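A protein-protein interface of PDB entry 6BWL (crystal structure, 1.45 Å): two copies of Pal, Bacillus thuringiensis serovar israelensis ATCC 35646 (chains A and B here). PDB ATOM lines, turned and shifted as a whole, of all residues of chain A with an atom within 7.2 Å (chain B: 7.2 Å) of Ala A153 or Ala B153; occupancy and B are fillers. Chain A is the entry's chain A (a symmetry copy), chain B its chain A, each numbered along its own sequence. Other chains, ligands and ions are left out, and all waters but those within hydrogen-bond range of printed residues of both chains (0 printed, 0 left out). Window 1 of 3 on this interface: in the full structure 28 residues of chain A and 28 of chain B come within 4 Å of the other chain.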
ATOM      1  N   PHE A  96       5.069  -4.411  -7.514  1.00  0.00           N
ATOM      2  CA  PHE A  96       5.905  -3.669  -8.456  1.00  0.00           C
ATOM      3  C   PHE A  96       5.540  -2.197  -8.538  1.00  0.00           C
ATOM      4  O   PHE A  96       6.406  -1.304  -8.565  1.00  0.00           O
ATOM      5  CB  PHE A  96       5.869  -4.373  -9.811  1.00  0.00           C
ATOM      6  CG  PHE A  96       6.585  -3.655 -10.920  1.00  0.00           C
ATOM      7  CD1 PHE A  96       7.973  -3.594 -10.936  1.00  0.00           C
ATOM      8  CD2 PHE A  96       5.880  -3.031 -11.960  1.00  0.00           C
ATOM      9  CE1 PHE A  96       8.616  -2.936 -11.967  1.00  0.00           C
ATOM     10  CE2 PHE A  96       6.514  -2.366 -12.975  1.00  0.00           C
ATOM     11  CZ  PHE A  96       7.904  -2.320 -12.964  1.00  0.00           C
ATOM     12  N   ASP A  99       6.377  -0.502  -5.181  1.00  0.00           N
ATOM     13  CA  ASP A  99       7.731  -0.517  -4.653  1.00  0.00           C
ATOM     14  C   ASP A  99       8.739  -0.046  -5.645  1.00  0.00           C
ATOM     15  O   ASP A  99       9.786   0.466  -5.213  1.00  0.00           O
ATOM     16  CB  ASP A  99       8.067  -1.908  -4.168  1.00  0.00           C
ATOM     17  CG  ASP A  99       7.268  -2.313  -2.939  1.00  0.00           C
ATOM     18  OD1 ASP A  99       6.346  -1.599  -2.539  1.00  0.00           O
ATOM     19  OD2 ASP A  99       7.588  -3.394  -2.345  1.00  0.00           O
ATOM     20  N   THR A 100       8.503  -0.238  -6.937  1.00  0.00           N
ATOM     21  CA  THR A 100       9.437   0.231  -7.961  1.00  0.00           C
ATOM     22  C   THR A 100       8.934   1.522  -8.580  1.00  0.00           C
ATOM     23  O   THR A 100       9.649   2.534  -8.560  1.00  0.00           O
ATOM     24  CB  THR A 100       9.688  -0.836  -9.038  1.00  0.00           C
ATOM     25  OG1 THR A 100      10.007  -2.096  -8.406  1.00  0.00           O
ATOM     26  CG2 THR A 100      10.774  -0.434  -9.962  1.00  0.00           C
ATOM     27  N   THR A 103       8.687   4.380  -6.004  1.00  0.00           N
ATOM     28  CA  THR A 103      10.018   4.903  -5.760  1.00  0.00           C
ATOM     29  C   THR A 103      10.462   5.854  -6.844  1.00  0.00           C
ATOM     30  O   THR A 103      11.014   6.939  -6.574  1.00  0.00           O
ATOM     31  CB  THR A 103      11.022   3.784  -5.560  1.00  0.00           C
ATOM     32  OG1 THR A 103      10.616   3.013  -4.408  1.00  0.00           O
ATOM     33  CG2 THR A 103      12.428   4.308  -5.359  1.00  0.00           C
ATOM     34  N   PHE A 119      16.701   5.433   0.661  1.00  0.00           N
ATOM     35  CA  PHE A 119      15.810   4.402   0.135  1.00  0.00           C
ATOM     36  C   PHE A 119      15.822   3.186   1.046  1.00  0.00           C
ATOM     37  O   PHE A 119      16.885   2.568   1.247  1.00  0.00           O
ATOM     38  CB  PHE A 119      16.188   3.958  -1.266  1.00  0.00           C
ATOM     39  CG  PHE A 119      15.314   2.824  -1.745  1.00  0.00           C
ATOM     40  CD1 PHE A 119      13.958   3.014  -1.817  1.00  0.00           C
ATOM     41  CD2 PHE A 119      15.800   1.598  -2.017  1.00  0.00           C
ATOM     42  CE1 PHE A 119      13.092   1.983  -2.131  1.00  0.00           C
ATOM     43  CE2 PHE A 119      14.967   0.566  -2.335  1.00  0.00           C
ATOM     44  CZ  PHE A 119      13.615   0.737  -2.389  1.00  0.00           C
ATOM     45  N   VAL A 125      16.803  -9.016  -0.374  1.00  0.00           N
ATOM     46  CA  VAL A 125      17.411  -8.941  -1.696  1.00  0.00           C
ATOM     47  C   VAL A 125      18.699  -9.755  -1.759  1.00  0.00           C
ATOM     48  O   VAL A 125      19.436  -9.694  -2.743  1.00  0.00           O
ATOM     49  CB  VAL A 125      17.715  -7.485  -2.096  1.00  0.00           C
ATOM     50  CG1 VAL A 125      16.455  -6.638  -2.012  1.00  0.00           C
ATOM     51  CG2 VAL A 125      18.812  -6.911  -1.211  1.00  0.00           C
ATOM     52  N   TYR A 147       8.522  -9.232  -4.518  1.00  0.00           N
ATOM     53  CA  TYR A 147       8.906  -8.215  -3.527  1.00  0.00           C
ATOM     54  C   TYR A 147      10.406  -7.928  -3.588  1.00  0.00           C
ATOM     55  O   TYR A 147      10.815  -6.759  -3.704  1.00  0.00           O
ATOM     56  CB  TYR A 147       8.495  -8.651  -2.111  1.00  0.00           C
ATOM     57  CG  TYR A 147       9.045  -7.798  -1.000  1.00  0.00           C
ATOM     58  CD1 TYR A 147       9.935  -8.317  -0.098  1.00  0.00           C
ATOM     59  CD2 TYR A 147       8.615  -6.494  -0.827  1.00  0.00           C
ATOM     60  CE1 TYR A 147      10.418  -7.538   0.939  1.00  0.00           C
ATOM     61  CE2 TYR A 147       9.063  -5.711   0.199  1.00  0.00           C
ATOM     62  CZ  TYR A 147       9.978  -6.243   1.073  1.00  0.00           C
ATOM     63  OH  TYR A 147      10.449  -5.497   2.144  1.00  0.00           O
ATOM     64  N   ALA A 148      11.212  -8.972  -3.491  1.00  0.00           N
ATOM     65  CA  ALA A 148      12.647  -8.778  -3.532  1.00  0.00           C
ATOM     66  C   ALA A 148      13.068  -8.167  -4.862  1.00  0.00           C
ATOM     67  O   ALA A 148      13.914  -7.266  -4.890  1.00  0.00           O
ATOM     68  CB  ALA A 148      13.379 -10.089  -3.296  1.00  0.00           C
ATOM     69  N   GLY A 149      12.496  -8.645  -5.974  1.00  0.00           N
ATOM     70  CA  GLY A 149      12.875  -8.082  -7.268  1.00  0.00           C
ATOM     71  C   GLY A 149      12.524  -6.602  -7.369  1.00  0.00           C
ATOM     72  O   GLY A 149      13.294  -5.816  -7.930  1.00  0.00           O
ATOM     73  N   SER A 150      11.342  -6.221  -6.865  1.00  0.00           N
ATOM     74  CA  SER A 150      10.870  -4.839  -6.927  1.00  0.00           C
ATOM     75  C   SER A 150      11.782  -3.939  -6.108  1.00  0.00           C
ATOM     76  O   SER A 150      12.032  -2.789  -6.477  1.00  0.00           O
ATOM     77  CB  SER A 150       9.428  -4.737  -6.444  1.00  0.00           C
ATOM     78  OG  SER A 150       8.493  -5.452  -7.255  1.00  0.00           O
ATOM     79  N   LYS A 151      12.269  -4.446  -4.970  1.00  0.00           N
ATOM     80  CA  LYS A 151      13.180  -3.671  -4.114  1.00  0.00           C
ATOM     81  C   LYS A 151      14.538  -3.483  -4.782  1.00  0.00           C
ATOM     82  O   LYS A 151      15.080  -2.383  -4.774  1.00  0.00           O
ATOM     83  CB  LYS A 151      13.314  -4.302  -2.727  1.00  0.00           C
ATOM     84  CG  LYS A 151      12.074  -4.065  -1.864  1.00  0.00           C
ATOM     85  CD  LYS A 151      11.968  -2.621  -1.380  1.00  0.00           C
ATOM     86  CE  LYS A 151      10.991  -2.439  -0.223  1.00  0.00           C
ATOM     87  NZ  LYS A 151      10.929  -1.041   0.260  1.00  0.00           N
ATOM     88  N   ILE A 152      15.064  -4.551  -5.386  1.00  0.00           N
ATOM     89  CA  ILE A 152      16.352  -4.417  -6.095  1.00  0.00           C
ATOM     90  C   ILE A 152      16.192  -3.452  -7.260  1.00  0.00           C
ATOM     91  O   ILE A 152      17.060  -2.621  -7.556  1.00  0.00           O
ATOM     92  CB  ILE A 152      16.880  -5.771  -6.581  1.00  0.00           C
ATOM     93  CG1 ILE A 152      17.279  -6.654  -5.399  1.00  0.00           C
ATOM     94  CG2 ILE A 152      18.092  -5.577  -7.474  1.00  0.00           C
ATOM     95  CD1 ILE A 152      17.394  -8.122  -5.730  1.00  0.00           C
ATOM     96  N   ALA A 153      15.046  -3.540  -7.948  1.00  0.00           N
ATOM     97  CA  ALA A 153      14.787  -2.654  -9.079  1.00  0.00           C
ATOM     98  C   ALA A 153      14.839  -1.189  -8.601  1.00  0.00           C
ATOM     99  O   ALA A 153      15.427  -0.319  -9.246  1.00  0.00           O
ATOM    100  CB  ALA A 153      13.449  -2.977  -9.734  1.00  0.00           C
ATOM    101  N   ALA A 154      14.165  -0.921  -7.486  1.00  0.00           N
ATOM    102  CA  ALA A 154      14.127   0.420  -6.913  1.00  0.00           C
ATOM    103  C   ALA A 154      15.529   0.874  -6.519  1.00  0.00           C
ATOM    104  O   ALA A 154      15.903   2.020  -6.813  1.00  0.00           O
ATOM    105  CB  ALA A 154      13.165   0.442  -5.747  1.00  0.00           C
ATOM    106  N   GLU A 155      16.295  -0.008  -5.866  1.00  0.00           N
ATOM    107  CA  GLU A 155      17.670   0.342  -5.480  1.00  0.00           C
ATOM    108  C   GLU A 155      18.457   0.867  -6.679  1.00  0.00           C
ATOM    109  O   GLU A 155      19.217   1.836  -6.577  1.00  0.00           O
ATOM    110  CB  GLU A 155      18.475  -0.848  -4.975  1.00  0.00           C
ATOM    111  CG  GLU A 155      18.030  -1.477  -3.680  1.00  0.00           C
ATOM    112  CD  GLU A 155      18.964  -2.568  -3.217  1.00  0.00           C
ATOM    113  OE1 GLU A 155      19.835  -2.968  -4.020  1.00  0.00           O
ATOM    114  OE2 GLU A 155      18.828  -3.077  -2.091  1.00  0.00           O
ATOM    115  N   ASN A 156      18.295   0.186  -7.807  1.00  0.00           N
ATOM    116  CA  ASN A 156      19.114   0.524  -8.963  1.00  0.00           C
ATOM    117  C   ASN A 156      18.685   1.788  -9.624  1.00  0.00           C
ATOM    118  O   ASN A 156      19.552   2.493 -10.155  1.00  0.00           O
ATOM    119  CB  ASN A 156      19.180  -0.663  -9.912  1.00  0.00           C
ATOM    120  CG  ASN A 156      20.179  -1.647  -9.418  1.00  0.00           C
ATOM    121  OD1 ASN A 156      21.358  -1.508  -9.737  1.00  0.00           O
ATOM    122  ND2 ASN A 156      19.762  -2.556  -8.538  1.00  0.00           N
ATOM    123  N   MET A 157      17.396   2.123  -9.607  1.00  0.00           N
ATOM    124  CA  MET A 157      16.999   3.447 -10.053  1.00  0.00           C
ATOM    125  C   MET A 157      17.555   4.537  -9.145  1.00  0.00           C
ATOM    126  O   MET A 157      18.098   5.546  -9.615  1.00  0.00           O
ATOM    127  CB  MET A 157      15.489   3.548 -10.196  1.00  0.00           C
ATOM    128  CG  MET A 157      14.914   2.600 -11.227  1.00  0.00           C
ATOM    129  SD  MET A 157      15.732   2.556 -12.832  1.00  0.00           S
ATOM    130  CE  MET A 157      15.538   4.262 -13.349  1.00  0.00           C
ATOM    131  N   VAL A 158      17.456   4.328  -7.833  1.00  0.00           N
ATOM    132  CA  VAL A 158      17.967   5.304  -6.869  1.00  0.00           C
ATOM    133  C   VAL A 158      19.466   5.545  -7.061  1.00  0.00           C
ATOM    134  O   VAL A 158      19.913   6.684  -7.164  1.00  0.00           O
ATOM    135  CB  VAL A 158      17.653   4.811  -5.442  1.00  0.00           C
ATOM    136  CG1 VAL A 158      18.363   5.678  -4.391  1.00  0.00           C
ATOM    137  CG2 VAL A 158      16.146   4.809  -5.205  1.00  0.00           C
ATOM    138  N   LEU A 159      20.234   4.465  -7.140  1.00  0.00           N
ATOM    139  CA  LEU A 159      21.680   4.606  -7.304  1.00  0.00           C
ATOM    140  C   LEU A 159      22.017   5.232  -8.656  1.00  0.00           C
ATOM    141  O   LEU A 159      22.979   6.010  -8.755  1.00  0.00           O
ATOM    142  CB  LEU A 159      22.406   3.294  -7.112  1.00  0.00           C
ATOM    143  CG  LEU A 159      22.413   2.824  -5.659  1.00  0.00           C
ATOM    144  CD1 LEU A 159      22.758   1.351  -5.601  1.00  0.00           C
ATOM    145  CD2 LEU A 159      23.365   3.652  -4.813  1.00  0.00           C
ATOM    146  N   PHE B  96      13.023   4.505 -18.197  1.00  0.00           N
ATOM    147  CA  PHE B  96      12.418   3.649 -17.178  1.00  0.00           C
ATOM    148  C   PHE B  96      11.128   2.995 -17.644  1.00  0.00           C
ATOM    149  O   PHE B  96      10.876   1.799 -17.414  1.00  0.00           O
ATOM    150  CB  PHE B  96      12.251   4.453 -15.890  1.00  0.00           C
ATOM    151  CG  PHE B  96      11.525   3.740 -14.784  1.00  0.00           C
ATOM    152  CD1 PHE B  96      12.134   2.692 -14.106  1.00  0.00           C
ATOM    153  CD2 PHE B  96      10.224   4.108 -14.410  1.00  0.00           C
ATOM    154  CE1 PHE B  96      11.455   2.052 -13.087  1.00  0.00           C
ATOM    155  CE2 PHE B  96       9.544   3.467 -13.410  1.00  0.00           C
ATOM    156  CZ  PHE B  96      10.178   2.419 -12.750  1.00  0.00           C
ATOM    157  N   ASP B  99      11.934   0.488 -20.457  1.00  0.00           N
ATOM    158  CA  ASP B  99      12.848  -0.619 -20.233  1.00  0.00           C
ATOM    159  C   ASP B  99      12.498  -1.416 -19.022  1.00  0.00           C
ATOM    160  O   ASP B  99      12.835  -2.612 -18.996  1.00  0.00           O
ATOM    161  CB  ASP B  99      14.261  -0.094 -20.138  1.00  0.00           C
ATOM    162  CG  ASP B  99      14.778   0.451 -21.460  1.00  0.00           C
ATOM    163  OD1 ASP B  99      14.013   0.571 -22.419  1.00  0.00           O
ATOM    164  OD2 ASP B  99      16.011   0.764 -21.540  1.00  0.00           O
ATOM    165  N   THR B 100      11.894  -0.808 -18.009  1.00  0.00           N
ATOM    166  CA  THR B 100      11.494  -1.542 -16.807  1.00  0.00           C
ATOM    167  C   THR B 100      10.009  -1.849 -16.848  1.00  0.00           C
ATOM    168  O   THR B 100       9.620  -3.022 -16.760  1.00  0.00           O
ATOM    169  CB  THR B 100      11.866  -0.782 -15.524  1.00  0.00           C
ATOM    170  OG1 THR B 100      13.248  -0.363 -15.592  1.00  0.00           O
ATOM    171  CG2 THR B 100      11.637  -1.608 -14.316  1.00  0.00           C
ATOM    172  N   THR B 103       9.066  -4.118 -19.820  1.00  0.00           N
ATOM    173  CA  THR B 103       9.436  -5.483 -19.498  1.00  0.00           C
ATOM    174  C   THR B 103       8.423  -6.153 -18.604  1.00  0.00           C
ATOM    175  O   THR B 103       8.026  -7.313 -18.822  1.00  0.00           O
ATOM    176  CB  THR B 103      10.830  -5.550 -18.903  1.00  0.00           C
ATOM    177  OG1 THR B 103      11.764  -5.040 -19.880  1.00  0.00           O
ATOM    178  CG2 THR B 103      11.215  -6.960 -18.510  1.00  0.00           C
ATOM    179  N   PHE B 119      15.377 -12.257 -21.733  1.00  0.00           N
ATOM    180  CA  PHE B 119      15.448 -10.821 -21.479  1.00  0.00           C
ATOM    181  C   PHE B 119      16.789 -10.273 -21.941  1.00  0.00           C
ATOM    182  O   PHE B 119      17.844 -10.704 -21.439  1.00  0.00           O
ATOM    183  CB  PHE B 119      15.266 -10.474 -20.013  1.00  0.00           C
ATOM    184  CG  PHE B 119      15.444  -8.996 -19.765  1.00  0.00           C
ATOM    185  CD1 PHE B 119      14.624  -8.109 -20.415  1.00  0.00           C
ATOM    186  CD2 PHE B 119      16.438  -8.501 -19.001  1.00  0.00           C
ATOM    187  CE1 PHE B 119      14.811  -6.742 -20.325  1.00  0.00           C
ATOM    188  CE2 PHE B 119      16.638  -7.157 -18.893  1.00  0.00           C
ATOM    189  CZ  PHE B 119      15.843  -6.265 -19.551  1.00  0.00           C
ATOM    190  N   VAL B 125      25.471  -2.852 -17.316  1.00  0.00           N
ATOM    191  CA  VAL B 125      25.058  -3.024 -15.929  1.00  0.00           C
ATOM    192  C   VAL B 125      26.236  -3.429 -15.049  1.00  0.00           C
ATOM    193  O   VAL B 125      26.061  -3.768 -13.879  1.00  0.00           O
ATOM    194  CB  VAL B 125      23.944  -4.079 -15.798  1.00  0.00           C
ATOM    195  CG1 VAL B 125      22.766  -3.720 -16.691  1.00  0.00           C
ATOM    196  CG2 VAL B 125      24.481  -5.461 -16.141  1.00  0.00           C
ATOM    197  N   TYR B 147      19.656   4.337 -17.848  1.00  0.00           N
ATOM    198  CA  TYR B 147      19.581   3.167 -18.736  1.00  0.00           C
ATOM    199  C   TYR B 147      20.056   1.904 -18.019  1.00  0.00           C
ATOM    200  O   TYR B 147      19.340   0.886 -18.005  1.00  0.00           O
ATOM    201  CB  TYR B 147      20.396   3.403 -20.018  1.00  0.00           C
ATOM    202  CG  TYR B 147      20.580   2.188 -20.886  1.00  0.00           C
ATOM    203  CD1 TYR B 147      21.824   1.651 -21.079  1.00  0.00           C
ATOM    204  CD2 TYR B 147      19.506   1.627 -21.557  1.00  0.00           C
ATOM    205  CE1 TYR B 147      21.993   0.548 -21.901  1.00  0.00           C
ATOM    206  CE2 TYR B 147      19.651   0.551 -22.386  1.00  0.00           C
ATOM    207  CZ  TYR B 147      20.903   0.011 -22.542  1.00  0.00           C
ATOM    208  OH  TYR B 147      21.107  -1.069 -23.389  1.00  0.00           O
ATOM    209  N   ALA B 148      21.250   1.958 -17.453  1.00  0.00           N
ATOM    210  CA  ALA B 148      21.772   0.796 -16.764  1.00  0.00           C
ATOM    211  C   ALA B 148      20.875   0.420 -15.591  1.00  0.00           C
ATOM    212  O   ALA B 148      20.606  -0.766 -15.371  1.00  0.00           O
ATOM    213  CB  ALA B 148      23.193   1.041 -16.285  1.00  0.00           C
ATOM    214  N   GLY B 149      20.407   1.413 -14.824  1.00  0.00           N
ATOM    215  CA  GLY B 149      19.542   1.090 -13.691  1.00  0.00           C
ATOM    216  C   GLY B 149      18.245   0.425 -14.137  1.00  0.00           C
ATOM    217  O   GLY B 149      17.763  -0.504 -13.480  1.00  0.00           O
ATOM    218  N   SER B 150      17.650   0.923 -15.231  1.00  0.00           N
ATOM    219  CA  SER B 150      16.386   0.400 -15.744  1.00  0.00           C
ATOM    220  C   SER B 150      16.564  -1.039 -16.202  1.00  0.00           C
ATOM    221  O   SER B 150      15.663  -1.867 -16.049  1.00  0.00           O
ATOM    222  CB  SER B 150      15.861   1.270 -16.879  1.00  0.00           C
ATOM    223  OG  SER B 150      15.540   2.607 -16.485  1.00  0.00           O
ATOM    224  N   LYS B 151      17.723  -1.346 -16.794  1.00  0.00           N
ATOM    225  CA  LYS B 151      18.010  -2.714 -17.253  1.00  0.00           C
ATOM    226  C   LYS B 151      18.193  -3.665 -16.073  1.00  0.00           C
ATOM    227  O   LYS B 151      17.652  -4.765 -16.081  1.00  0.00           O
ATOM    228  CB  LYS B 151      19.215  -2.745 -18.196  1.00  0.00           C
ATOM    229  CG  LYS B 151      18.873  -2.200 -19.583  1.00  0.00           C
ATOM    230  CD  LYS B 151      18.005  -3.163 -20.390  1.00  0.00           C
ATOM    231  CE  LYS B 151      17.974  -2.845 -21.881  1.00  0.00           C
ATOM    232  NZ  LYS B 151      17.160  -3.809 -22.655  1.00  0.00           N
ATOM    233  N   ILE B 152      18.928  -3.220 -15.051  1.00  0.00           N
ATOM    234  CA  ILE B 152      19.096  -4.074 -13.859  1.00  0.00           C
ATOM    235  C   ILE B 152      17.745  -4.292 -13.195  1.00  0.00           C
ATOM    236  O   ILE B 152      17.407  -5.384 -12.724  1.00  0.00           O
ATOM    237  CB  ILE B 152      20.099  -3.478 -12.865  1.00  0.00           C
ATOM    238  CG1 ILE B 152      21.512  -3.492 -13.446  1.00  0.00           C
ATOM    239  CG2 ILE B 152      20.097  -4.270 -11.571  1.00  0.00           C
ATOM    240  CD1 ILE B 152      22.477  -2.557 -12.758  1.00  0.00           C
ATOM    241  N   ALA B 153      16.927  -3.232 -13.158  1.00  0.00           N
ATOM    242  CA  ALA B 153      15.602  -3.335 -12.552  1.00  0.00           C
ATOM    243  C   ALA B 153      14.791  -4.424 -13.282  1.00  0.00           C
ATOM    244  O   ALA B 153      14.120  -5.253 -12.665  1.00  0.00           O
ATOM    245  CB  ALA B 153      14.880  -1.992 -12.581  1.00  0.00           C
ATOM    246  N   ALA B 154      14.820  -4.374 -14.611  1.00  0.00           N
ATOM    247  CA  ALA B 154      14.103  -5.342 -15.435  1.00  0.00           C
ATOM    248  C   ALA B 154      14.633  -6.750 -15.188  1.00  0.00           C
ATOM    249  O   ALA B 154      13.830  -7.684 -15.036  1.00  0.00           O
ATOM    250  CB  ALA B 154      14.200  -4.935 -16.888  1.00  0.00           C
ATOM    251  N   GLU B 155      15.962  -6.905 -15.146  1.00  0.00           N
ATOM    252  CA  GLU B 155      16.551  -8.226 -14.881  1.00  0.00           C
ATOM    253  C   GLU B 155      15.954  -8.846 -13.619  1.00  0.00           C
ATOM    254  O   GLU B 155      15.659 -10.044 -13.567  1.00  0.00           O
ATOM    255  CB  GLU B 155      18.050  -8.176 -14.622  1.00  0.00           C
ATOM    256  CG  GLU B 155      18.931  -7.763 -15.772  1.00  0.00           C
ATOM    257  CD  GLU B 155      20.400  -7.860 -15.438  1.00  0.00           C
ATOM    258  OE1 GLU B 155      20.713  -8.046 -14.242  1.00  0.00           O
ATOM    259  OE2 GLU B 155      21.258  -7.709 -16.325  1.00  0.00           O
ATOM    260  N   ASN B 156      15.822  -8.019 -12.589  1.00  0.00           N
ATOM    261  CA  ASN B 156      15.400  -8.552 -11.301  1.00  0.00           C
ATOM    262  C   ASN B 156      13.948  -8.887 -11.263  1.00  0.00           C
ATOM    263  O   ASN B 156      13.586  -9.842 -10.565  1.00  0.00           O
ATOM    264  CB  ASN B 156      15.833  -7.613 -10.187  1.00  0.00           C
ATOM    265  CG  ASN B 156      17.269  -7.834  -9.872  1.00  0.00           C
ATOM    266  OD1 ASN B 156      17.573  -8.706  -9.062  1.00  0.00           O
ATOM    267  ND2 ASN B 156      18.166  -7.162 -10.594  1.00  0.00           N
ATOM    268  N   MET B 157      13.098  -8.164 -11.990  1.00  0.00           N
ATOM    269  CA  MET B 157      11.723  -8.611 -12.132  1.00  0.00           C
ATOM    270  C   MET B 157      11.637  -9.934 -12.885  1.00  0.00           C
ATOM    271  O   MET B 157      10.928 -10.861 -12.469  1.00  0.00           O
ATOM    272  CB  MET B 157      10.860  -7.539 -12.776  1.00  0.00           C
ATOM    273  CG  MET B 157      10.774  -6.263 -11.964  1.00  0.00           C
ATOM    274  SD  MET B 157      10.410  -6.444 -10.209  1.00  0.00           S
ATOM    275  CE  MET B 157       8.818  -7.267 -10.284  1.00  0.00           C
ATOM    276  N   VAL B 158      12.385 -10.046 -13.981  1.00  0.00           N
ATOM    277  CA  VAL B 158      12.388 -11.275 -14.775  1.00  0.00           C
ATOM    278  C   VAL B 158      12.832 -12.478 -13.938  1.00  0.00           C
ATOM    279  O   VAL B 158      12.162 -13.507 -13.909  1.00  0.00           O
ATOM    280  CB  VAL B 158      13.297 -11.077 -16.004  1.00  0.00           C
ATOM    281  CG1 VAL B 158      13.516 -12.403 -16.746  1.00  0.00           C
ATOM    282  CG2 VAL B 158      12.697 -10.032 -16.940  1.00  0.00           C
ATOM    283  N   LEU B 159      13.948 -12.329 -13.234  1.00  0.00           N
ATOM    284  CA  LEU B 159      14.453 -13.436 -12.423  1.00  0.00           C
ATOM    285  C   LEU B 159      13.494 -13.755 -11.277  1.00  0.00           C
ATOM    286  O   LEU B 159      13.335 -14.930 -10.911  1.00  0.00           O
ATOM    287  CB  LEU B 159      15.851 -13.175 -11.911  1.00  0.00           C
ATOM    288  CG  LEU B 159      16.908 -13.232 -13.010  1.00  0.00           C
ATOM    289  CD1 LEU B 159      18.178 -12.557 -12.533  1.00  0.00           C
ATOM    290  CD2 LEU B 159      17.172 -14.661 -13.453  1.00  0.00           C
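Thr A100 touches none of the printed residues of chain B.
Val A125 touches none of the printed residues of chain B.
Printed residues of chain B within 4 Å of Gly A149: Asn B156 (3.8 Å) and Met B157 (3.5 Å).
Printed residues of chain B within 4 Å of Ser A150: Met B157.
Ala A153 touches one residue of chain B.
Ala B153 touches just one residue of chain A: Ala A153 (3.3 Å).
The nearest printed residue of chain B that does not touch Gly A149 is Ala B153 (4.8 Å).
Phe A96 touches Met B157, and with the chains exchanged Met A157 touches Phe B96.
Gly A149 touches Asn B156, and with the chains exchanged Asn A156 touches Gly B149.
Ile A152 touches Asn B156, and with the chains exchanged Asn A156 touches Ile B152.
Ala A153 touches its own counterpart, Ala B153.
Positions printed for both chains: 96, 99, 100, 103, 119, 125, 147, 148, 149, 150, 151, 152, 153, 154, 155, 156, 157, 158 and 159.
SD of Met B157 lies close to O of Gly A149 (3.7 Å).
The side-chain sulfur (SD) of Met A157 sits close to the backbone carbonyl oxygen (O) of Gly B149 (3.7 Å).
The backbone NH of Ser B150 lies within hydrogen-bond range of the side-chain sulfur of Met A157, at 3.5 Å.
SD of Met B157 is in hydrogen-bond range of N of Ser A150.
Met B157 touches Phe A96 (SD to CD1, 3.8 Å).
Gly A149 touches Asn B156 (CA to O, 3.8 Å).
OD1 of Asn B156 touches CD1 of Ile A152, at 3.4 Å.
Ala B153 touches Ala A153.
CA of Gly B149 touches O of Asn A156, 3.8 Å away.
OD1 of Asn A156 touches CD1 of Ile B152, 3.4 Å away.
Met A157 touches Phe B96 (SD to CD1, 3.8 Å).
Printed residues of chain B that touch a printed residue of chain A: Phe B96, Gly B149, Ser B150, Ile B152, Ala B153, Asn B156 and Met B157.
Hydrophobic or aromatic side chains of chain B within 4 Å of the printed part of chain A: Phe B96, Ile B152, Ala B153 and Met B157.
Among the printed residues, 11 pairs touch across the chains.
Among the printed residues, no Asp or Glu carboxylate lies within 4 Å of a Lys or Arg side-chain nitrogen of the other chain.
The side-chain hydroxyl of Thr B100 sits at hydrogen-bond distance from the backbone carbonyl oxygen of Ser B150 (2.9 Å).
The side-chain amide nitrogen (ND2) of Asn B156 sits at hydrogen-bond distance from the backbone carbonyl oxygen (O) of Ile B152 (2.9 Å).
OG1 of Thr A100 sits at hydrogen-bond distance from O of Ser A150, at 2.9 Å.
The side-chain amide nitrogen of Asn A156 sits at hydrogen-bond distance from the backbone carbonyl oxygen of Ile A152, 2.9 Å away.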
